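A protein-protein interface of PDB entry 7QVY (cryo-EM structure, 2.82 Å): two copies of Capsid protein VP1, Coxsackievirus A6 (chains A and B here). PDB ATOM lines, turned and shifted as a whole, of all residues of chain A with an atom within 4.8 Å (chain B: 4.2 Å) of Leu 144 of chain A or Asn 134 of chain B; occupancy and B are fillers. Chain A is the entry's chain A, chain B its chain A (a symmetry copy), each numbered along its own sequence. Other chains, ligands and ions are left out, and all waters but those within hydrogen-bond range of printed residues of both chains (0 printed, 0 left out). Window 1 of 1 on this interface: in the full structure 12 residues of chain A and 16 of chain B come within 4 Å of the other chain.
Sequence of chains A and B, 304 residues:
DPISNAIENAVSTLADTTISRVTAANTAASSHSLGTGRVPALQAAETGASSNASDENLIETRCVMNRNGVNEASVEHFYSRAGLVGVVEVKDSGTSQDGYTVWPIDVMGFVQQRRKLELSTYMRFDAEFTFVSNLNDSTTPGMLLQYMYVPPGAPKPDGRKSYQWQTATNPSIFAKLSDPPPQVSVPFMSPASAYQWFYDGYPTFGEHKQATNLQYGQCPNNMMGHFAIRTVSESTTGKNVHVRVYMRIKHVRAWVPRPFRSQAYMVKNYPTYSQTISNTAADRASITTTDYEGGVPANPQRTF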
ATOM      1  N   GLY A 142      15.131  -4.926 -17.064  1.00  0.00           N
ATOM      2  CA  GLY A 142      14.620  -5.414 -18.357  1.00  0.00           C
ATOM      3  C   GLY A 142      14.078  -4.307 -19.247  1.00  0.00           C
ATOM      4  O   GLY A 142      13.335  -4.646 -20.167  1.00  0.00           O
ATOM      5  N   MET A 143      14.455  -3.043 -19.044  1.00  0.00           N
ATOM      6  CA  MET A 143      13.854  -1.919 -19.795  1.00  0.00           C
ATOM      7  C   MET A 143      14.252  -2.024 -21.268  1.00  0.00           C
ATOM      8  O   MET A 143      15.394  -2.347 -21.565  1.00  0.00           O
ATOM      9  CB  MET A 143      14.295  -0.570 -19.235  1.00  0.00           C
ATOM     10  CG  MET A 143      13.761  -0.294 -17.840  1.00  0.00           C
ATOM     11  SD  MET A 143      14.588   1.134 -17.087  1.00  0.00           S
ATOM     12  CE  MET A 143      14.544   2.299 -18.444  1.00  0.00           C
ATOM     13  N   LEU A 144      13.312  -1.773 -22.166  1.00  0.00           N
ATOM     14  CA  LEU A 144      13.563  -1.757 -23.621  1.00  0.00           C
ATOM     15  C   LEU A 144      14.090  -0.380 -24.026  1.00  0.00           C
ATOM     16  O   LEU A 144      13.649   0.656 -23.472  1.00  0.00           O
ATOM     17  CB  LEU A 144      12.268  -2.084 -24.361  1.00  0.00           C
ATOM     18  CG  LEU A 144      12.438  -2.565 -25.798  1.00  0.00           C
ATOM     19  CD1 LEU A 144      13.456  -3.682 -25.881  1.00  0.00           C
ATOM     20  CD2 LEU A 144      11.112  -3.034 -26.349  1.00  0.00           C
ATOM     21  N   LEU A 145      15.017  -0.367 -24.967  1.00  0.00           N
ATOM     22  CA  LEU A 145      15.589   0.880 -25.509  1.00  0.00           C
ATOM     23  C   LEU A 145      15.594   0.800 -27.027  1.00  0.00           C
ATOM     24  O   LEU A 145      15.714  -0.295 -27.596  1.00  0.00           O
ATOM     25  CB  LEU A 145      17.010   1.076 -24.992  1.00  0.00           C
ATOM     26  CG  LEU A 145      17.163   1.533 -23.544  1.00  0.00           C
ATOM     27  CD1 LEU A 145      18.616   1.502 -23.143  1.00  0.00           C
ATOM     28  CD2 LEU A 145      16.665   2.937 -23.322  1.00  0.00           C
ATOM     29  N   GLN A 146      15.482   1.950 -27.668  1.00  0.00           N
ATOM     30  CA  GLN A 146      15.595   2.062 -29.129  1.00  0.00           C
ATOM     31  C   GLN A 146      16.767   2.984 -29.442  1.00  0.00           C
ATOM     32  O   GLN A 146      16.748   4.132 -29.016  1.00  0.00           O
ATOM     33  CB  GLN A 146      14.308   2.605 -29.717  1.00  0.00           C
ATOM     34  CG  GLN A 146      14.358   2.618 -31.234  1.00  0.00           C
ATOM     35  CD  GLN A 146      13.153   3.267 -31.863  1.00  0.00           C
ATOM     36  OE1 GLN A 146      12.166   3.585 -31.189  1.00  0.00           O
ATOM     37  NE2 GLN A 146      13.239   3.478 -33.165  1.00  0.00           N
ATOM     38  N   PHE A 174      16.728  -2.347 -31.250  1.00  0.00           N
ATOM     39  CA  PHE A 174      15.894  -2.586 -30.057  1.00  0.00           C
ATOM     40  C   PHE A 174      16.649  -3.558 -29.165  1.00  0.00           C
ATOM     41  O   PHE A 174      16.929  -4.715 -29.587  1.00  0.00           O
ATOM     42  CB  PHE A 174      14.530  -3.110 -30.473  1.00  0.00           C
ATOM     43  CG  PHE A 174      13.652  -2.049 -31.056  1.00  0.00           C
ATOM     44  CD1 PHE A 174      12.866  -1.275 -30.230  1.00  0.00           C
ATOM     45  CD2 PHE A 174      13.620  -1.836 -32.421  1.00  0.00           C
ATOM     46  CE1 PHE A 174      12.019  -0.325 -30.772  1.00  0.00           C
ATOM     47  CE2 PHE A 174      12.795  -0.868 -32.959  1.00  0.00           C
ATOM     48  CZ  PHE A 174      11.996  -0.122 -32.128  1.00  0.00           C
ATOM     49  N   ALA A 175      17.003  -3.098 -27.979  1.00  0.00           N
ATOM     50  CA  ALA A 175      17.827  -3.871 -27.041  1.00  0.00           C
ATOM     51  C   ALA A 175      17.439  -3.504 -25.626  1.00  0.00           C
ATOM     52  O   ALA A 175      17.002  -2.372 -25.395  1.00  0.00           O
ATOM     53  CB  ALA A 175      19.266  -3.582 -27.301  1.00  0.00           C
ATOM     54  N   LYS A 176      17.620  -4.440 -24.710  1.00  0.00           N
ATOM     55  CA  LYS A 176      17.314  -4.223 -23.282  1.00  0.00           C
ATOM     56  C   LYS A 176      18.597  -3.923 -22.506  1.00  0.00           C
ATOM     57  O   LYS A 176      19.706  -4.281 -22.996  1.00  0.00           O
ATOM     58  CB  LYS A 176      16.612  -5.459 -22.744  1.00  0.00           C
ATOM     59  CG  LYS A 176      15.596  -6.070 -23.689  1.00  0.00           C
ATOM     60  CD  LYS A 176      14.724  -7.062 -22.959  1.00  0.00           C
ATOM     61  CE  LYS A 176      13.661  -7.689 -23.832  1.00  0.00           C
ATOM     62  NZ  LYS A 176      14.209  -8.842 -24.583  1.00  0.00           N
ATOM     63  N   ARG A 230      15.973   6.424 -26.941  1.00  0.00           N
ATOM     64  CA  ARG A 230      14.810   6.595 -26.046  1.00  0.00           C
ATOM     65  C   ARG A 230      14.477   5.291 -25.331  1.00  0.00           C
ATOM     66  O   ARG A 230      14.869   4.231 -25.798  1.00  0.00           O
ATOM     67  CB  ARG A 230      13.627   7.058 -26.884  1.00  0.00           C
ATOM     68  CG  ARG A 230      12.909   5.922 -27.586  1.00  0.00           C
ATOM     69  CD  ARG A 230      11.788   6.480 -28.381  1.00  0.00           C
ATOM     70  NE  ARG A 230      11.198   5.476 -29.242  1.00  0.00           N
ATOM     71  CZ  ARG A 230       9.899   5.378 -29.511  1.00  0.00           C
ATOM     72  NH1 ARG A 230       9.022   6.191 -28.947  1.00  0.00           N
ATOM     73  NH2 ARG A 230       9.484   4.428 -30.324  1.00  0.00           N
ATOM     74  N   THR A 231      13.699   5.377 -24.268  1.00  0.00           N
ATOM     75  CA  THR A 231      13.027   4.206 -23.660  1.00  0.00           C
ATOM     76  C   THR A 231      11.716   3.989 -24.393  1.00  0.00           C
ATOM     77  O   THR A 231      10.990   4.963 -24.592  1.00  0.00           O
ATOM     78  CB  THR A 231      12.806   4.420 -22.165  1.00  0.00           C
ATOM     79  OG1 THR A 231      12.091   5.641 -21.953  1.00  0.00           O
ATOM     80  CG2 THR A 231      14.119   4.507 -21.427  1.00  0.00           C
ATOM     81  N   VAL A 232      11.405   2.761 -24.769  1.00  0.00           N
ATOM     82  CA  VAL A 232      10.134   2.487 -25.498  1.00  0.00           C
ATOM     83  C   VAL A 232       9.011   2.417 -24.467  1.00  0.00           C
ATOM     84  O   VAL A 232       8.723   1.338 -24.006  1.00  0.00           O
ATOM     85  CB  VAL A 232      10.224   1.201 -26.325  1.00  0.00           C
ATOM     86  CG1 VAL A 232       8.969   0.991 -27.138  1.00  0.00           C
ATOM     87  CG2 VAL A 232      11.434   1.223 -27.227  1.00  0.00           C
ATOM     88  N   VAL B 132       8.074  -6.594 -31.176  1.00  0.00           N
ATOM     89  CA  VAL B 132       8.819  -5.882 -30.114  1.00  0.00           C
ATOM     90  C   VAL B 132       7.793  -5.590 -29.027  1.00  0.00           C
ATOM     91  O   VAL B 132       7.095  -4.556 -29.063  1.00  0.00           O
ATOM     92  CB  VAL B 132       9.508  -4.623 -30.655  1.00  0.00           C
ATOM     93  CG1 VAL B 132      10.315  -3.960 -29.577  1.00  0.00           C
ATOM     94  CG2 VAL B 132      10.385  -4.921 -31.853  1.00  0.00           C
ATOM     95  N   SER B 133       7.708  -6.481 -28.054  1.00  0.00           N
ATOM     96  CA  SER B 133       6.668  -6.432 -27.006  1.00  0.00           C
ATOM     97  C   SER B 133       7.279  -5.973 -25.695  1.00  0.00           C
ATOM     98  O   SER B 133       8.362  -6.437 -25.356  1.00  0.00           O
ATOM     99  CB  SER B 133       6.003  -7.767 -26.872  1.00  0.00           C
ATOM    100  OG  SER B 133       5.537  -8.226 -28.135  1.00  0.00           O
ATOM    101  N   ASN B 134       6.564  -5.135 -24.967  1.00  0.00           N
ATOM    102  CA  ASN B 134       6.995  -4.687 -23.624  1.00  0.00           C
ATOM    103  C   ASN B 134       5.774  -4.162 -22.889  1.00  0.00           C
ATOM    104  O   ASN B 134       4.692  -4.146 -23.476  1.00  0.00           O
ATOM    105  CB  ASN B 134       8.108  -3.645 -23.720  1.00  0.00           C
ATOM    106  CG  ASN B 134       7.704  -2.417 -24.500  1.00  0.00           C
ATOM    107  OD1 ASN B 134       6.966  -2.488 -25.483  1.00  0.00           O
ATOM    108  ND2 ASN B 134       8.198  -1.278 -24.086  1.00  0.00           N
ATOM    109  N   LEU B 135       5.950  -3.730 -21.650  1.00  0.00           N
ATOM    110  CA  LEU B 135       4.844  -3.194 -20.828  1.00  0.00           C
ATOM    111  C   LEU B 135       4.768  -1.679 -21.020  1.00  0.00           C
ATOM    112  O   LEU B 135       5.480  -1.148 -21.896  1.00  0.00           O
ATOM    113  CB  LEU B 135       5.079  -3.595 -19.373  1.00  0.00           C
ATOM    114  CG  LEU B 135       5.001  -5.087 -19.042  1.00  0.00           C
ATOM    115  CD1 LEU B 135       4.842  -5.273 -17.550  1.00  0.00           C
ATOM    116  CD2 LEU B 135       3.853  -5.785 -19.756  1.00  0.00           C
ATOM    117  N   SER B 138       8.130   0.329 -20.349  1.00  0.00           N
ATOM    118  CA  SER B 138       9.270  -0.332 -21.036  1.00  0.00           C
ATOM    119  C   SER B 138       9.770  -1.579 -20.292  1.00  0.00           C
ATOM    120  O   SER B 138      10.715  -2.160 -20.786  1.00  0.00           O
ATOM    121  CB  SER B 138      10.393   0.649 -21.312  1.00  0.00           C
ATOM    122  OG  SER B 138      11.093   1.014 -20.134  1.00  0.00           O
ATOM    123  N   THR B 139       9.128  -2.035 -19.222  1.00  0.00           N
ATOM    124  CA  THR B 139       9.562  -3.233 -18.470  1.00  0.00           C
ATOM    125  C   THR B 139       9.277  -4.480 -19.314  1.00  0.00           C
ATOM    126  O   THR B 139       8.229  -4.530 -19.997  1.00  0.00           O
ATOM    127  CB  THR B 139       8.862  -3.295 -17.108  1.00  0.00           C
ATOM    128  OG1 THR B 139       9.002  -2.019 -16.478  1.00  0.00           O
ATOM    129  CG2 THR B 139       9.409  -4.386 -16.215  1.00  0.00           C
ATOM    130  N   THR B 140      10.140  -5.481 -19.222  1.00  0.00           N
ATOM    131  CA  THR B 140       9.964  -6.780 -19.926  1.00  0.00           C
ATOM    132  C   THR B 140      10.094  -7.909 -18.911  1.00  0.00           C
ATOM    133  O   THR B 140      11.150  -8.532 -18.804  1.00  0.00           O
ATOM    134  CB  THR B 140      10.948  -6.912 -21.095  1.00  0.00           C
ATOM    135  OG1 THR B 140      12.284  -6.868 -20.601  1.00  0.00           O
ATOM    136  CG2 THR B 140      10.804  -5.818 -22.126  1.00  0.00           C
ATOM    137  N   LEU B 177       8.536 -11.911 -22.723  1.00  0.00           N
ATOM    138  CA  LEU B 177       9.004 -10.510 -22.849  1.00  0.00           C
ATOM    139  C   LEU B 177      10.515 -10.449 -22.597  1.00  0.00           C
ATOM    140  O   LEU B 177      11.165  -9.617 -23.241  1.00  0.00           O
ATOM    141  CB  LEU B 177       8.239  -9.605 -21.880  1.00  0.00           C
ATOM    142  CG  LEU B 177       6.754  -9.426 -22.193  1.00  0.00           C
ATOM    143  CD1 LEU B 177       6.095  -8.509 -21.164  1.00  0.00           C
ATOM    144  CD2 LEU B 177       6.569  -8.883 -23.598  1.00  0.00           C
ATOM    145  N   VAL B 241       0.187  -5.022 -22.506  1.00  0.00           N
ATOM    146  CA  VAL B 241       1.397  -5.333 -23.314  1.00  0.00           C
ATOM    147  C   VAL B 241       1.283  -4.583 -24.636  1.00  0.00           C
ATOM    148  O   VAL B 241       0.307  -4.820 -25.380  1.00  0.00           O
ATOM    149  CB  VAL B 241       1.534  -6.846 -23.531  1.00  0.00           C
ATOM    150  CG1 VAL B 241       2.739  -7.187 -24.388  1.00  0.00           C
ATOM    151  CG2 VAL B 241       1.571  -7.578 -22.204  1.00  0.00           C
ATOM    152  N   HIS B 242       2.263  -3.744 -24.940  1.00  0.00           N
ATOM    153  CA  HIS B 242       2.351  -3.049 -26.246  1.00  0.00           C
ATOM    154  C   HIS B 242       3.210  -3.882 -27.180  1.00  0.00           C
ATOM    155  O   HIS B 242       4.367  -4.147 -26.848  1.00  0.00           O
ATOM    156  CB  HIS B 242       2.909  -1.642 -26.083  1.00  0.00           C
ATOM    157  CG  HIS B 242       2.179  -0.863 -25.046  1.00  0.00           C
ATOM    158  ND1 HIS B 242       1.021  -0.148 -25.333  1.00  0.00           N
ATOM    159  CD2 HIS B 242       2.408  -0.718 -23.713  1.00  0.00           C
ATOM    160  CE1 HIS B 242       0.586   0.424 -24.222  1.00  0.00           C
ATOM    161  NE2 HIS B 242       1.417   0.085 -23.216  1.00  0.00           N
ATOM    162  N   ARG B 244       4.881  -3.971 -30.895  1.00  0.00           N
ATOM    163  CA  ARG B 244       5.260  -3.283 -32.139  1.00  0.00           C
ATOM    164  C   ARG B 244       5.583  -4.349 -33.179  1.00  0.00           C
ATOM    165  O   ARG B 244       6.574  -5.096 -33.010  1.00  0.00           O
ATOM    166  CB  ARG B 244       6.463  -2.386 -31.886  1.00  0.00           C
ATOM    167  CG  ARG B 244       6.089  -1.034 -31.321  1.00  0.00           C
ATOM    168  CD  ARG B 244       7.284  -0.332 -30.722  1.00  0.00           C
ATOM    169  NE  ARG B 244       6.903   0.987 -30.224  1.00  0.00           N
ATOM    170  CZ  ARG B 244       6.294   1.251 -29.047  1.00  0.00           C
ATOM    171  NH1 ARG B 244       5.974   0.294 -28.171  1.00  0.00           N
ATOM    172  NH2 ARG B 244       6.027   2.515 -28.742  1.00  0.00           N
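Printed residues of chain B within 4 Å of Leu 144 of chain A: Val 132, Asn 134 and Ser 138.
Gln 146 of chain A touches none of the printed residues of chain B.
Of the printed residues of chain B, Phe 174 of chain A touches Val 132 (3.8 Å).
Printed residues of chain B within 4 Å of Lys 176 of chain A: Thr 140 (3.4 Å) and Leu 177 (3.2 Å).
Asn 134 of chain B touches just these residues of chain A: Leu 144 (3.9 Å) and Val 232 (2.7 Å).
His 242 of chain B touches none of the printed residues of chain A.
The nearest printed residue of chain B that does not touch Leu 144 of chain A is Ser 133 of chain B (4.5 Å).
The nearest printed residue of chain A that does not touch Asn 134 of chain B is Thr 231 of chain A (6.3 Å).
The backbone NH of Val 232 of chain A lies within hydrogen-bond range of the backbone carbonyl oxygen of Leu 144 of chain A, 3.3 Å away.
The backbone NH (N) of Val 132 of chain B lies within hydrogen-bond range of the backbone carbonyl oxygen (O) of Arg 244 of chain B, 2.8 Å away.
The backbone carbonyl oxygen of Asn 134 of chain B lies within hydrogen-bond range of the backbone NH of His 242 of chain B, 2.9 Å away.
Among the printed residues, merely in contact across the chains: Val 232 of chain A with Ser 138 of chain B (3.2 Å), Val 232 of chain A with Arg 244 of chain B (3.2 Å), Met 143 of chain A with Ser 138 of chain B (3.3 Å), Lys 176 of chain A with Thr 140 of chain B (3.4 Å), Leu 144 of chain A with Val 132 of chain B (3.5 Å), Gly 142 of chain A with Ser 138 of chain B (3.7 Å), Phe 174 of chain A with Val 132 of chain B (3.8 Å) and Leu 144 of chain A with Asn 134 of chain B (3.9 Å).
Of the 11 printed residues of chain A, 6 touch a printed residue of chain B.
Hydrophobic or aromatic side chains of chain A that line the printed part of chain B: Met 143, Leu 144, Phe 174 and Val 232.
Printed residues of chain B that touch a printed residue of chain A: Val 132, Asn 134, Ser 138, Thr 140, Leu 177 and Arg 244.
Among the printed residues, 12 pairs touch across the chains.
Among the printed residues, no Asp or Glu carboxylate lies within 4 Å of a Lys or Arg side-chain nitrogen of the other chain.
No position is printed for both chains.
Of the 12 pairs that touch across the chains among the printed residues, none has its exchanged pair printed and touching as well.
The backbone carbonyl oxygen of Gly 142 of chain A is in hydrogen-bond range of the side-chain hydroxyl of Thr 140 of chain B (2.5 Å).
N of Leu 144 of chain A sits at hydrogen-bond distance from O of Ser 138 of chain B (3.0 Å).
The backbone carbonyl oxygen (O) of Leu 177 of chain B sits close to the side-chain amino group (NZ) of Lys 176 of chain A, 3.4 Å away.
The side-chain amide nitrogen (ND2) of Asn 134 of chain B is in hydrogen-bond range of the backbone carbonyl oxygen (O) of Val 232 of chain A, 2.7 Å away.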
